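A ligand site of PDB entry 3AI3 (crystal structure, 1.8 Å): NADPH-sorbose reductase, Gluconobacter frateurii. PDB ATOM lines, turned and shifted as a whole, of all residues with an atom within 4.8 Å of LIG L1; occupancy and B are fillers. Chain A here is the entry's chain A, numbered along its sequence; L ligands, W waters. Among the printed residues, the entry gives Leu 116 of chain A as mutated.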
ATOM      1  N   GLY A  14      18.481 -21.836 -11.695  1.00  0.00           N
ATOM      2  CA  GLY A  14      19.042 -23.121 -11.218  1.00  0.00           C
ATOM      3  C   GLY A  14      20.026 -22.935 -10.080  1.00  0.00           C
ATOM      4  O   GLY A  14      21.153 -23.460 -10.097  1.00  0.00           O
ATOM      5  N   SER A  15      19.631 -22.155  -9.066  1.00  0.00           N
ATOM      6  CA  SER A  15      20.587 -21.710  -8.088  1.00  0.00           C
ATOM      7  C   SER A  15      20.364 -22.225  -6.697  1.00  0.00           C
ATOM      8  O   SER A  15      20.931 -21.663  -5.752  1.00  0.00           O
ATOM      9  CB  SER A  15      20.728 -20.175  -8.053  1.00  0.00           C
ATOM     10  OG  SER A  15      19.442 -19.540  -8.038  1.00  0.00           O
ATOM     11  N   SER A  16      19.572 -23.284  -6.561  1.00  0.00           N
ATOM     12  CA  SER A  16      19.318 -23.873  -5.257  1.00  0.00           C
ATOM     13  C   SER A  16      20.365 -24.916  -4.912  1.00  0.00           C
ATOM     14  O   SER A  16      20.486 -25.332  -3.748  1.00  0.00           O
ATOM     15  CB  SER A  16      17.910 -24.462  -5.168  1.00  0.00           C
ATOM     16  OG  SER A  16      17.771 -25.534  -6.069  1.00  0.00           O
ATOM     17  N   SER A  17      21.153 -25.316  -5.915  1.00  0.00           N
ATOM     18  CA  SER A  17      22.245 -26.288  -5.690  1.00  0.00           C
ATOM     19  C   SER A  17      23.302 -26.256  -6.793  1.00  0.00           C
ATOM     20  O   SER A  17      23.134 -25.521  -7.795  1.00  0.00           O
ATOM     21  CB  SER A  17      21.695 -27.698  -5.511  1.00  0.00           C
ATOM     22  OG  SER A  17      20.881 -28.028  -6.601  1.00  0.00           O
ATOM     23  N   GLY A  18      24.374 -27.044  -6.590  1.00  0.00           N
ATOM     24  CA  GLY A  18      25.439 -27.191  -7.597  1.00  0.00           C
ATOM     25  C   GLY A  18      26.108 -25.878  -7.993  1.00  0.00           C
ATOM     26  O   GLY A  18      26.372 -25.006  -7.136  1.00  0.00           O
ATOM     27  N   ILE A  19      26.390 -25.739  -9.285  1.00  0.00           N
ATOM     28  CA  ILE A  19      27.105 -24.563  -9.801  1.00  0.00           C
ATOM     29  C   ILE A  19      26.319 -23.291  -9.520  1.00  0.00           C
ATOM     30  O   ILE A  19      26.884 -22.283  -9.098  1.00  0.00           O
ATOM     31  CB  ILE A  19      27.383 -24.723 -11.316  1.00  0.00           C
ATOM     32  CG1 ILE A  19      28.344 -25.880 -11.537  1.00  0.00           C
ATOM     33  CG2 ILE A  19      27.900 -23.402 -11.944  1.00  0.00           C
ATOM     34  CD1 ILE A  19      28.447 -26.335 -13.014  1.00  0.00           C
ATOM     35  N   GLY A  20      25.014 -23.326  -9.713  1.00  0.00           N
ATOM     36  CA  GLY A  20      24.232 -22.086  -9.592  1.00  0.00           C
ATOM     37  C   GLY A  20      24.232 -21.544  -8.168  1.00  0.00           C
ATOM     38  O   GLY A  20      24.242 -20.329  -7.937  1.00  0.00           O
ATOM     39  N   VAL A  37      16.306 -18.948  -8.426  1.00  0.00           N
ATOM     40  CA  VAL A  37      15.238 -19.570  -9.214  1.00  0.00           C
ATOM     41  C   VAL A  37      15.520 -21.058  -9.318  1.00  0.00           C
ATOM     42  O   VAL A  37      16.606 -21.443  -9.728  1.00  0.00           O
ATOM     43  CB  VAL A  37      15.199 -19.055 -10.664  1.00  0.00           C
ATOM     44  CG1 VAL A  37      13.979 -19.626 -11.388  1.00  0.00           C
ATOM     45  CG2 VAL A  37      15.186 -17.521 -10.717  1.00  0.00           C
ATOM     46  N   ALA A  38      14.534 -21.880  -8.986  1.00  0.00           N
ATOM     47  CA  ALA A  38      14.635 -23.337  -9.113  1.00  0.00           C
ATOM     48  C   ALA A  38      13.227 -23.904  -8.914  1.00  0.00           C
ATOM     49  O   ALA A  38      12.308 -23.168  -8.617  1.00  0.00           O
ATOM     50  CB  ALA A  38      15.601 -23.932  -8.081  1.00  0.00           C
ATOM     51  N   ARG A  39      13.081 -25.214  -9.042  1.00  0.00           N
ATOM     52  CA  ARG A  39      11.768 -25.822  -8.941  1.00  0.00           C
ATOM     53  C   ARG A  39      11.363 -26.188  -7.524  1.00  0.00           C
ATOM     54  O   ARG A  39      10.231 -25.916  -7.129  1.00  0.00           O
ATOM     55  CB  ARG A  39      11.679 -27.035  -9.862  1.00  0.00           C
ATOM     56  CG  ARG A  39      11.652 -26.629 -11.343  1.00  0.00           C
ATOM     57  CD  ARG A  39      11.814 -27.838 -12.217  1.00  0.00           C
ATOM     58  NE  ARG A  39      13.066 -28.530 -11.924  1.00  0.00           N
ATOM     59  CZ  ARG A  39      13.489 -29.599 -12.581  1.00  0.00           C
ATOM     60  NH1 ARG A  39      12.753 -30.094 -13.574  1.00  0.00           N
ATOM     61  NH2 ARG A  39      14.628 -30.179 -12.251  1.00  0.00           N
ATOM     62  N   GLN A  40      12.267 -26.809  -6.771  1.00  0.00           N
ATOM     63  CA  GLN A  40      11.953 -27.268  -5.387  1.00  0.00           C
ATOM     64  C   GLN A  40      11.994 -26.164  -4.330  1.00  0.00           C
ATOM     65  O   GLN A  40      13.017 -25.488  -4.147  1.00  0.00           O
ATOM     66  CB  GLN A  40      12.853 -28.436  -4.980  1.00  0.00           C
ATOM     67  CG  GLN A  40      12.717 -29.619  -5.911  1.00  0.00           C
ATOM     68  CD  GLN A  40      11.480 -30.456  -5.654  1.00  0.00           C
ATOM     69  OE1 GLN A  40      10.339 -30.002  -5.834  1.00  0.00           O
ATOM     70  NE2 GLN A  40      11.687 -31.702  -5.257  1.00  0.00           N
ATOM     71  N   ARG A  43      14.791 -26.579  -1.052  1.00  0.00           N
ATOM     72  CA  ARG A  43      16.183 -26.228  -1.312  1.00  0.00           C
ATOM     73  C   ARG A  43      16.318 -24.724  -1.513  1.00  0.00           C
ATOM     74  O   ARG A  43      17.264 -24.097  -1.034  1.00  0.00           O
ATOM     75  CB  ARG A  43      16.688 -26.987  -2.548  1.00  0.00           C
ATOM     76  CG  ARG A  43      16.831 -28.473  -2.306  1.00  0.00           C
ATOM     77  CD  ARG A  43      16.544 -29.316  -3.543  1.00  0.00           C
ATOM     78  NE  ARG A  43      17.456 -29.073  -4.648  1.00  0.00           N
ATOM     79  CZ  ARG A  43      17.242 -29.469  -5.902  1.00  0.00           C
ATOM     80  NH1 ARG A  43      18.121 -29.216  -6.858  1.00  0.00           N
ATOM     81  NH2 ARG A  43      16.119 -30.125  -6.206  1.00  0.00           N
ATOM     82  N   VAL A  64       9.886 -21.853  -9.745  1.00  0.00           N
ATOM     83  CA  VAL A  64       9.225 -22.077 -11.030  1.00  0.00           C
ATOM     84  C   VAL A  64      10.075 -22.959 -11.955  1.00  0.00           C
ATOM     85  O   VAL A  64      11.262 -23.191 -11.709  1.00  0.00           O
ATOM     86  CB  VAL A  64       8.948 -20.735 -11.778  1.00  0.00           C
ATOM     87  CG1 VAL A  64       7.935 -19.869 -11.030  1.00  0.00           C
ATOM     88  CG2 VAL A  64      10.226 -19.990 -11.988  1.00  0.00           C
ATOM     89  N   ASP A  65       9.434 -23.416 -13.036  1.00  0.00           N
ATOM     90  CA  ASP A  65      10.094 -24.172 -14.099  1.00  0.00           C
ATOM     91  C   ASP A  65      10.475 -23.204 -15.234  1.00  0.00           C
ATOM     92  O   ASP A  65       9.606 -22.699 -15.941  1.00  0.00           O
ATOM     93  CB  ASP A  65       9.127 -25.277 -14.585  1.00  0.00           C
ATOM     94  CG  ASP A  65       9.729 -26.187 -15.645  1.00  0.00           C
ATOM     95  OD1 ASP A  65      10.834 -25.908 -16.160  1.00  0.00           O
ATOM     96  OD2 ASP A  65       9.070 -27.183 -15.989  1.00  0.00           O
ATOM     97  N   VAL A  66      11.778 -22.914 -15.386  1.00  0.00           N
ATOM     98  CA  VAL A  66      12.196 -21.921 -16.370  1.00  0.00           C
ATOM     99  C   VAL A  66      12.147 -22.475 -17.797  1.00  0.00           C
ATOM    100  O   VAL A  66      12.386 -21.758 -18.752  1.00  0.00           O
ATOM    101  CB  VAL A  66      13.616 -21.286 -16.077  1.00  0.00           C
ATOM    102  CG1 VAL A  66      13.648 -20.568 -14.750  1.00  0.00           C
ATOM    103  CG2 VAL A  66      14.711 -22.323 -16.151  1.00  0.00           C
ATOM    104  N   ALA A  67      11.846 -23.774 -17.930  1.00  0.00           N
ATOM    105  CA  ALA A  67      11.648 -24.385 -19.236  1.00  0.00           C
ATOM    106  C   ALA A  67      10.283 -24.030 -19.848  1.00  0.00           C
ATOM    107  O   ALA A  67       9.946 -24.484 -20.939  1.00  0.00           O
ATOM    108  CB  ALA A  67      11.846 -25.918 -19.164  1.00  0.00           C
ATOM    109  N   ASN A  92      21.730 -20.640 -15.957  1.00  0.00           N
ATOM    110  CA  ASN A  92      22.474 -21.787 -15.474  1.00  0.00           C
ATOM    111  C   ASN A  92      21.608 -23.042 -15.349  1.00  0.00           C
ATOM    112  O   ASN A  92      22.133 -24.146 -15.412  1.00  0.00           O
ATOM    113  CB  ASN A  92      23.119 -21.415 -14.141  1.00  0.00           C
ATOM    114  CG  ASN A  92      23.547 -22.632 -13.347  1.00  0.00           C
ATOM    115  OD1 ASN A  92      22.772 -23.145 -12.517  1.00  0.00           O
ATOM    116  ND2 ASN A  92      24.749 -23.114 -13.594  1.00  0.00           N
ATOM    117  N   ALA A  93      20.292 -22.890 -15.185  1.00  0.00           N
ATOM    118  CA  ALA A  93      19.426 -24.081 -15.065  1.00  0.00           C
ATOM    119  C   ALA A  93      19.624 -25.039 -16.231  1.00  0.00           C
ATOM    120  O   ALA A  93      19.548 -24.644 -17.390  1.00  0.00           O
ATOM    121  CB  ALA A  93      17.953 -23.672 -14.944  1.00  0.00           C
ATOM    122  N   GLY A  94      19.863 -26.304 -15.926  1.00  0.00           N
ATOM    123  CA  GLY A  94      20.087 -27.263 -16.973  1.00  0.00           C
ATOM    124  C   GLY A  94      20.437 -28.610 -16.380  1.00  0.00           C
ATOM    125  O   GLY A  94      20.643 -28.754 -15.183  1.00  0.00           O
ATOM    126  N   THR A  95      20.533 -29.592 -17.258  1.00  0.00           N
ATOM    127  CA  THR A  95      20.921 -30.933 -16.833  1.00  0.00           C
ATOM    128  C   THR A  95      21.485 -31.646 -18.038  1.00  0.00           C
ATOM    129  O   THR A  95      21.197 -31.242 -19.175  1.00  0.00           O
ATOM    130  CB  THR A  95      19.706 -31.713 -16.254  1.00  0.00           C
ATOM    131  OG1 THR A  95      20.166 -32.966 -15.729  1.00  0.00           O
ATOM    132  CG2 THR A  95      18.629 -31.964 -17.316  1.00  0.00           C
ATOM    133  N   LEU A 115      14.558 -25.918 -22.261  1.00  0.00           N
ATOM    134  CA  LEU A 115      15.284 -25.733 -20.997  1.00  0.00           C
ATOM    135  C   LEU A 115      16.556 -24.924 -21.179  1.00  0.00           C
ATOM    136  O   LEU A 115      16.829 -23.990 -20.415  1.00  0.00           O
ATOM    137  CB  LEU A 115      15.630 -27.105 -20.383  1.00  0.00           C
ATOM    138  CG  LEU A 115      16.588 -27.091 -19.171  1.00  0.00           C
ATOM    139  CD1 LEU A 115      15.987 -26.307 -18.014  1.00  0.00           C
ATOM    140  CD2 LEU A 115      16.947 -28.525 -18.770  1.00  0.00           C
ATOM    141  N   LEU A 116      17.340 -25.302 -22.180  1.00  0.00           N
ATOM    142  CA  LEU A 116      18.682 -24.730 -22.333  1.00  0.00           C
ATOM    143  C   LEU A 116      18.709 -23.509 -23.235  1.00  0.00           C
ATOM    144  O   LEU A 116      19.503 -22.569 -23.017  1.00  0.00           O
ATOM    145  CB  LEU A 116      19.650 -25.788 -22.857  1.00  0.00           C
ATOM    146  CG  LEU A 116      19.839 -27.024 -21.963  1.00  0.00           C
ATOM    147  CD1 LEU A 116      20.760 -28.097 -22.553  1.00  0.00           C
ATOM    148  CD2 LEU A 116      20.305 -26.632 -20.572  1.00  0.00           C
ATOM    149  N   ASN A 142      25.793 -20.136 -19.051  1.00  0.00           N
ATOM    150  CA  ASN A 142      26.589 -21.299 -18.661  1.00  0.00           C
ATOM    151  C   ASN A 142      26.216 -22.378 -19.652  1.00  0.00           C
ATOM    152  O   ASN A 142      25.168 -23.016 -19.513  1.00  0.00           O
ATOM    153  CB  ASN A 142      26.226 -21.724 -17.223  1.00  0.00           C
ATOM    154  CG  ASN A 142      26.993 -22.950 -16.729  1.00  0.00           C
ATOM    155  OD1 ASN A 142      26.826 -23.364 -15.580  1.00  0.00           O
ATOM    156  ND2 ASN A 142      27.808 -23.531 -17.572  1.00  0.00           N
ATOM    157  N   ALA A 143      27.047 -22.547 -20.678  1.00  0.00           N
ATOM    158  CA  ALA A 143      26.811 -23.615 -21.628  1.00  0.00           C
ATOM    159  C   ALA A 143      27.577 -24.865 -21.168  1.00  0.00           C
ATOM    160  O   ALA A 143      27.173 -25.471 -20.184  1.00  0.00           O
ATOM    161  CB  ALA A 143      27.177 -23.191 -23.045  1.00  0.00           C
ATOM    162  N   SER A 144      28.688 -25.205 -21.805  1.00  0.00           N
ATOM    163  CA  SER A 144      29.438 -26.419 -21.435  1.00  0.00           C
ATOM    164  C   SER A 144      30.580 -26.588 -22.427  1.00  0.00           C
ATOM    165  O   SER A 144      30.462 -26.174 -23.570  1.00  0.00           O
ATOM    166  CB  SER A 144      28.547 -27.664 -21.574  1.00  0.00           C
ATOM    167  OG  SER A 144      29.311 -28.839 -21.362  1.00  0.00           O
ATOM    168  N   TYR A 157      21.980 -32.922 -25.441  1.00  0.00           N
ATOM    169  CA  TYR A 157      22.709 -31.896 -24.679  1.00  0.00           C
ATOM    170  C   TYR A 157      23.755 -31.176 -25.536  1.00  0.00           C
ATOM    171  O   TYR A 157      23.862 -29.930 -25.466  1.00  0.00           O
ATOM    172  CB  TYR A 157      23.382 -32.594 -23.509  1.00  0.00           C
ATOM    173  CG  TYR A 157      24.144 -31.737 -22.528  1.00  0.00           C
ATOM    174  CD1 TYR A 157      23.479 -31.097 -21.481  1.00  0.00           C
ATOM    175  CD2 TYR A 157      25.538 -31.645 -22.592  1.00  0.00           C
ATOM    176  CE1 TYR A 157      24.194 -30.354 -20.513  1.00  0.00           C
ATOM    177  CE2 TYR A 157      26.252 -30.897 -21.638  1.00  0.00           C
ATOM    178  CZ  TYR A 157      25.566 -30.268 -20.607  1.00  0.00           C
ATOM    179  OH  TYR A 157      26.274 -29.555 -19.659  1.00  0.00           O
ATOM    180  N   LYS A 161      23.324 -27.257 -26.133  1.00  0.00           N
ATOM    181  CA  LYS A 161      24.397 -26.405 -25.592  1.00  0.00           C
ATOM    182  C   LYS A 161      25.127 -25.627 -26.692  1.00  0.00           C
ATOM    183  O   LYS A 161      25.466 -24.459 -26.496  1.00  0.00           O
ATOM    184  CB  LYS A 161      25.371 -27.199 -24.729  1.00  0.00           C
ATOM    185  CG  LYS A 161      24.730 -27.622 -23.392  1.00  0.00           C
ATOM    186  CD  LYS A 161      24.528 -26.408 -22.430  1.00  0.00           C
ATOM    187  CE  LYS A 161      24.243 -26.889 -21.006  1.00  0.00           C
ATOM    188  NZ  LYS A 161      24.155 -25.725 -20.009  1.00  0.00           N
ATOM    189  N   PRO A 187      32.033 -24.714 -18.919  1.00  0.00           N
ATOM    190  CA  PRO A 187      32.760 -25.512 -17.918  1.00  0.00           C
ATOM    191  C   PRO A 187      33.089 -26.890 -18.396  1.00  0.00           C
ATOM    192  O   PRO A 187      32.372 -27.453 -19.243  1.00  0.00           O
ATOM    193  CB  PRO A 187      31.766 -25.623 -16.743  1.00  0.00           C
ATOM    194  CG  PRO A 187      30.849 -24.374 -16.942  1.00  0.00           C
ATOM    195  CD  PRO A 187      30.685 -24.370 -18.453  1.00  0.00           C
ATOM    196  N   GLY A 188      34.179 -27.415 -17.825  1.00  0.00           N
ATOM    197  CA  GLY A 188      34.566 -28.822 -17.970  1.00  0.00           C
ATOM    198  C   GLY A 188      33.945 -29.637 -16.851  1.00  0.00           C
ATOM    199  O   GLY A 188      32.785 -29.408 -16.490  1.00  0.00           O
ATOM    200  N   LEU A 189      34.696 -30.587 -16.319  1.00  0.00           N
ATOM    201  CA  LEU A 189      34.188 -31.462 -15.270  1.00  0.00           C
ATOM    202  C   LEU A 189      34.107 -30.682 -13.951  1.00  0.00           C
ATOM    203  O   LEU A 189      35.130 -30.340 -13.369  1.00  0.00           O
ATOM    204  CB  LEU A 189      35.143 -32.620 -15.056  1.00  0.00           C
ATOM    205  CG  LEU A 189      35.463 -33.488 -16.278  1.00  0.00           C
ATOM    206  CD1 LEU A 189      36.529 -34.533 -15.869  1.00  0.00           C
ATOM    207  CD2 LEU A 189      34.184 -34.158 -16.783  1.00  0.00           C
ATOM    208  N   ILE A 190      32.900 -30.451 -13.479  1.00  0.00           N
ATOM    209  CA  ILE A 190      32.675 -29.760 -12.200  1.00  0.00           C
ATOM    210  C   ILE A 190      31.973 -30.709 -11.237  1.00  0.00           C
ATOM    211  O   ILE A 190      30.923 -31.259 -11.558  1.00  0.00           O
ATOM    212  CB  ILE A 190      31.759 -28.488 -12.367  1.00  0.00           C
ATOM    213  CG1 ILE A 190      32.096 -27.702 -13.661  1.00  0.00           C
ATOM    214  CG2 ILE A 190      31.828 -27.584 -11.088  1.00  0.00           C
ATOM    215  CD1 ILE A 190      33.549 -27.159 -13.777  1.00  0.00           C
ATOM    216  N   THR A 192      29.579 -32.001  -9.000  1.00  0.00           N
ATOM    217  CA  THR A 192      28.239 -31.634  -8.533  1.00  0.00           C
ATOM    218  C   THR A 192      27.509 -32.925  -8.186  1.00  0.00           C
ATOM    219  O   THR A 192      28.019 -34.014  -8.503  1.00  0.00           O
ATOM    220  CB  THR A 192      27.474 -30.886  -9.641  1.00  0.00           C
ATOM    221  OG1 THR A 192      27.549 -31.663 -10.842  1.00  0.00           O
ATOM    222  CG2 THR A 192      28.102 -29.492  -9.873  1.00  0.00           C
ATOM    223  N   PRO A 193      26.325 -32.836  -7.537  1.00  0.00           N
ATOM    224  CA  PRO A 193      25.713 -34.047  -6.970  1.00  0.00           C
ATOM    225  C   PRO A 193      25.374 -35.157  -7.972  1.00  0.00           C
ATOM    226  O   PRO A 193      25.524 -36.338  -7.630  1.00  0.00           O
ATOM    227  CB  PRO A 193      24.413 -33.518  -6.313  1.00  0.00           C
ATOM    228  CG  PRO A 193      24.742 -32.079  -5.958  1.00  0.00           C
ATOM    229  CD  PRO A 193      25.649 -31.597  -7.065  1.00  0.00           C
ATOM    230  N   ASP A 194      24.961 -34.813  -9.196  1.00  0.00           N
ATOM    231  CA  ASP A 194      24.622 -35.838 -10.179  1.00  0.00           C
ATOM    232  C   ASP A 194      25.828 -36.682 -10.590  1.00  0.00           C
ATOM    233  O   ASP A 194      25.661 -37.848 -10.950  1.00  0.00           O
ATOM    234  CB  ASP A 194      23.926 -35.251 -11.420  1.00  0.00           C
ATOM    235  CG  ASP A 194      22.441 -34.905 -11.152  1.00  0.00           C
ATOM    236  OD1 ASP A 194      21.930 -35.177 -10.049  1.00  0.00           O
ATOM    237  OD2 ASP A 194      21.786 -34.388 -12.073  1.00  0.00           O
ATOM    238  N   TRP A 195      27.021 -36.103 -10.541  1.00  0.00           N
ATOM    239  CA  TRP A 195      28.236 -36.863 -10.857  1.00  0.00           C
ATOM    240  C   TRP A 195      28.432 -37.947  -9.810  1.00  0.00           C
ATOM    241  O   TRP A 195      28.805 -39.078 -10.134  1.00  0.00           O
ATOM    242  CB  TRP A 195      29.474 -35.963 -10.880  1.00  0.00           C
ATOM    243  CG  TRP A 195      29.723 -35.279 -12.191  1.00  0.00           C
ATOM    244  CD1 TRP A 195      29.620 -33.939 -12.461  1.00  0.00           C
ATOM    245  CD2 TRP A 195      30.120 -35.910 -13.408  1.00  0.00           C
ATOM    246  NE1 TRP A 195      29.955 -33.704 -13.785  1.00  0.00           N
ATOM    247  CE2 TRP A 195      30.270 -34.892 -14.385  1.00  0.00           C
ATOM    248  CE3 TRP A 195      30.397 -37.237 -13.763  1.00  0.00           C
ATOM    249  CZ2 TRP A 195      30.652 -35.172 -15.705  1.00  0.00           C
ATOM    250  CZ3 TRP A 195      30.787 -37.507 -15.087  1.00  0.00           C
ATOM    251  CH2 TRP A 195      30.909 -36.481 -16.033  1.00  0.00           C
HETATM  252  P1  LIG L   1      22.529 -29.450 -10.675  1.00  0.00           P
HETATM  253  O1  LIG L   1      23.362 -29.630  -9.472  1.00  0.00           O
HETATM  254  O2  LIG L   1      21.511 -30.449 -11.038  1.00  0.00           O
HETATM  255  O3  LIG L   1      21.763 -28.082 -10.436  1.00  0.00           O
HETATM  256  C1  LIG L   1      20.814 -27.651 -11.367  1.00  0.00           C
HETATM  257  C2  LIG L   1      20.039 -26.498 -10.733  1.00  0.00           C
HETATM  258  O4  LIG L   1      19.089 -26.096 -11.707  1.00  0.00           O
HETATM  259  C3  LIG L   1      19.241 -26.921  -9.506  1.00  0.00           C
HETATM  260  O5  LIG L   1      19.110 -25.828  -8.607  1.00  0.00           O
HETATM  261  C4  LIG L   1      17.878 -27.277 -10.060  1.00  0.00           C
HETATM  262  O6  LIG L   1      16.900 -27.164  -9.044  1.00  0.00           O
HETATM  263  C5  LIG L   1      17.763 -26.269 -11.200  1.00  0.00           C
HETATM  264  N1  LIG L   1      16.890 -26.632 -12.315  1.00  0.00           N
HETATM  265  C6  LIG L   1      16.959 -27.731 -13.142  1.00  0.00           C
HETATM  266  N2  LIG L   1      15.948 -27.654 -14.020  1.00  0.00           N
HETATM  267  C7  LIG L   1      15.240 -26.536 -13.778  1.00  0.00           C
HETATM  268  C8  LIG L   1      14.113 -25.982 -14.369  1.00  0.00           C
HETATM  269  N3  LIG L   1      13.512 -26.595 -15.398  1.00  0.00           N
HETATM  270  N4  LIG L   1      13.604 -24.804 -13.860  1.00  0.00           N
HETATM  271  C9  LIG L   1      14.203 -24.157 -12.802  1.00  0.00           C
HETATM  272  N5  LIG L   1      15.314 -24.736 -12.210  1.00  0.00           N
HETATM  273  C10 LIG L   1      15.811 -25.889 -12.706  1.00  0.00           C
HETATM  274  O7  LIG L   1      23.416 -29.136 -11.972  1.00  0.00           O
HETATM  275  P2  LIG L   1      24.850 -28.436 -12.206  1.00  0.00           P
HETATM  276  O8  LIG L   1      25.734 -29.572 -12.528  1.00  0.00           O
HETATM  277  O9  LIG L   1      25.100 -27.394 -11.191  1.00  0.00           O
HETATM  278  O10 LIG L   1      24.582 -27.721 -13.615  1.00  0.00           O
HETATM  279  C11 LIG L   1      24.137 -26.379 -13.766  1.00  0.00           C
HETATM  280  C12 LIG L   1      24.551 -26.003 -15.187  1.00  0.00           C
HETATM  281  O11 LIG L   1      25.935 -26.236 -15.398  1.00  0.00           O
HETATM  282  C13 LIG L   1      23.780 -26.788 -16.231  1.00  0.00           C
HETATM  283  O12 LIG L   1      23.369 -25.847 -17.226  1.00  0.00           O
HETATM  284  C14 LIG L   1      24.833 -27.708 -16.807  1.00  0.00           C
HETATM  285  O13 LIG L   1      24.581 -28.000 -18.166  1.00  0.00           O
HETATM  286  C15 LIG L   1      26.098 -26.845 -16.663  1.00  0.00           C
HETATM  287  N6  LIG L   1      27.337 -27.628 -16.668  1.00  0.00           N
HETATM  288  C16 LIG L   1      27.611 -28.485 -15.612  1.00  0.00           C
HETATM  289  C17 LIG L   1      28.803 -29.174 -15.631  1.00  0.00           C
HETATM  290  C18 LIG L   1      29.090 -30.162 -14.554  1.00  0.00           C
HETATM  291  O14 LIG L   1      30.134 -31.016 -14.799  1.00  0.00           O
HETATM  292  N7  LIG L   1      28.345 -30.228 -13.447  1.00  0.00           N
HETATM  293  C19 LIG L   1      29.705 -29.044 -16.711  1.00  0.00           C
HETATM  294  C20 LIG L   1      29.418 -28.162 -17.754  1.00  0.00           C
HETATM  295  C21 LIG L   1      28.228 -27.445 -17.693  1.00  0.00           C
HETATM  296  P3  LIG L   1      15.470 -27.895  -9.134  1.00  0.00           P
HETATM  297  O15 LIG L   1      15.550 -29.334  -9.559  1.00  0.00           O
HETATM  298  O16 LIG L   1      14.711 -27.175 -10.231  1.00  0.00           O
HETATM  299  O17 LIG L   1      14.796 -27.642  -7.816  1.00  0.00           O
HETATM  300  C1  LG2 L   2      30.370 -32.148 -18.890  1.00  0.00           C
HETATM  301  O1  LG2 L   2      31.218 -30.997 -18.883  1.00  0.00           O
HETATM  302  C2  LG2 L   2      28.932 -31.776 -19.179  1.00  0.00           C
HETATM  303  O2  LG2 L   2      28.621 -30.606 -19.440  1.00  0.00           O
HETATM  304  C3  LG2 L   2      27.914 -32.890 -19.201  1.00  0.00           C
HETATM  305  O3  LG2 L   2      28.582 -34.168 -19.222  1.00  0.00           O
HETATM  306  C4  LG2 L   2      26.905 -32.992 -18.050  1.00  0.00           C
HETATM  307  O4  LG2 L   2      25.594 -32.959 -18.618  1.00  0.00           O
HETATM  308  C5  LG2 L   2      26.977 -32.001 -16.883  1.00  0.00           C
HETATM  309  O5  LG2 L   2      25.763 -31.228 -16.779  1.00  0.00           O
HETATM  310  C6  LG2 L   2      27.197 -32.756 -15.574  1.00  0.00           C
HETATM  311  O6  LG2 L   2      26.067 -33.583 -15.263  1.00  0.00           O
HETATM  312  O   HOH W   1      15.255 -26.436  -5.603  1.00  0.00           O
HETATM  313  O   HOH W   2      24.357 -32.255 -10.277  1.00  0.00           O
HETATM  314  O   HOH W   3      23.423 -25.455 -10.631  1.00  0.00           O
HETATM  315  O   HOH W   4      22.354 -23.529 -19.483  1.00  0.00           O
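O16 of LIG L1 lies within hydrogen-bond range of N of Arg 39 (2.8 Å). The guanidinium group (NE) of Arg 39 is in salt-bridge range of an oxygen (O16) of LIG L1. An oxygen (O13) of LIG L1 lies within hydrogen-bond range of the side-chain hydroxyl (OH) of Tyr 157. O of Asn 92 sits at hydrogen-bond distance from O12 of LIG L1 (2.8 Å). O9 of LIG L1 is in hydrogen-bond range of N of Ile 19 (2.8 Å). O17 of LIG L1 lies within hydrogen-bond range of N of Gln 40, at 2.9 Å. The side-chain carboxylate (OD1) of Asp 65 lies within hydrogen-bond range of a nitrogen (N3) of LIG L1 (2.9 Å). An oxygen (O14) of LIG L1 lies within hydrogen-bond range of the indole nitrogen (NE1) of Trp 195 (2.9 Å). The backbone NH of Ser 16 sits at hydrogen-bond distance from an oxygen (O5) of LIG L1, 3.3 Å away. OG of Ser 16 sits at hydrogen-bond distance from O5 of LIG L1 (2.9 Å). NZ of Lys 161 is in hydrogen-bond range of O12 of LIG L1, 2.9 Å away. O11 of LIG L1 sits close to OD1 of Asn 142, at 3.0 Å. O of Gly 14 lies close to O5 of LIG L1. The backbone NH (N) of Val 66 is in hydrogen-bond range of a nitrogen (N4) of LIG L1 (3.0 Å). OG1 of Thr 192 lies within hydrogen-bond range of N7 of LIG L1 (3.1 Å). An oxygen (O14) of LIG L1 is in hydrogen-bond range of the backbone NH (N) of Ile 190, 3.1 Å away. O of Ile 190 lies within hydrogen-bond range of N7 of LIG L1, at 3.4 Å. NH2 of Arg 43 lies within salt-bridge range of O17 of LIG L1. The backbone NH of Ser 17 lies within hydrogen-bond range of an oxygen (O5) of LIG L1. OG of Ser 17 is in hydrogen-bond range of O5 of LIG L1, 3.5 Å away. The side-chain hydroxyl of Tyr 157 sits at hydrogen-bond distance from an oxygen (O2) of LG2 L2 (2.6 Å). An oxygen (O1) of LG2 L2 is in hydrogen-bond range of the backbone carbonyl oxygen (O) of Gly 188 (3.3 Å). OG of Ser 144 sits at hydrogen-bond distance from O2 of LG2 L2 (2.7 Å).
The side-chain amide nitrogen (ND2) of Asn 92 sits at hydrogen-bond distance from the side-chain amide oxygen (OD1) of Asn 142 (2.9 Å). The backbone carbonyl oxygen (O) of Gly 14 sits close to the side-chain amide oxygen (OD1) of Asn 92, 2.9 Å away. The side-chain carboxylate of Asp 65 is in hydrogen-bond range of the backbone NH of Ala 67 (3.0 Å). NZ of Lys 161 lies within hydrogen-bond range of O of Asn 142 (2.9 Å). The backbone carbonyl oxygen (O) of Val 37 lies within hydrogen-bond range of the backbone NH (N) of Gly 14 (2.7 Å). OG1 of Thr 192 is in hydrogen-bond range of O of Ile 190 (3.5 Å). The backbone NH (N) of Val 64 is in hydrogen-bond range of the backbone carbonyl oxygen (O) of Ala 38 (3.0 Å). O of Val 37 is in hydrogen-bond range of N of Ser 15, 3.2 Å away.
Residues that only touch LIG L1: Gly 188, Val 64, Ala 143, Pro 187, Ala 38, Gly 94, Leu 115, Gly 18, Ser 144, Ser 15, Ala 93 and Pro 193. Hydrophobic or aromatic side chains that line LIG L1: Ile 19, Ala 38, Val 66, Ala 93, Leu 115, Tyr 157, Pro 187, Ile 190, Pro 193 and Trp 195.
Water W1 lies within hydrogen-bond range of O17 of LIG L1, OG of Ser 16 and O of Gln 40. Water W2 lies within hydrogen-bond range of N of Asp 194 (2.8 Å), O1 of LIG L1 (2.9 Å) and OG1 of Thr 192 (3.3 Å). Water W4 lies within hydrogen-bond range of the backbone carbonyl oxygen of Asn 142, the side-chain amino group of Lys 161 and an oxygen (O12) of LIG L1.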
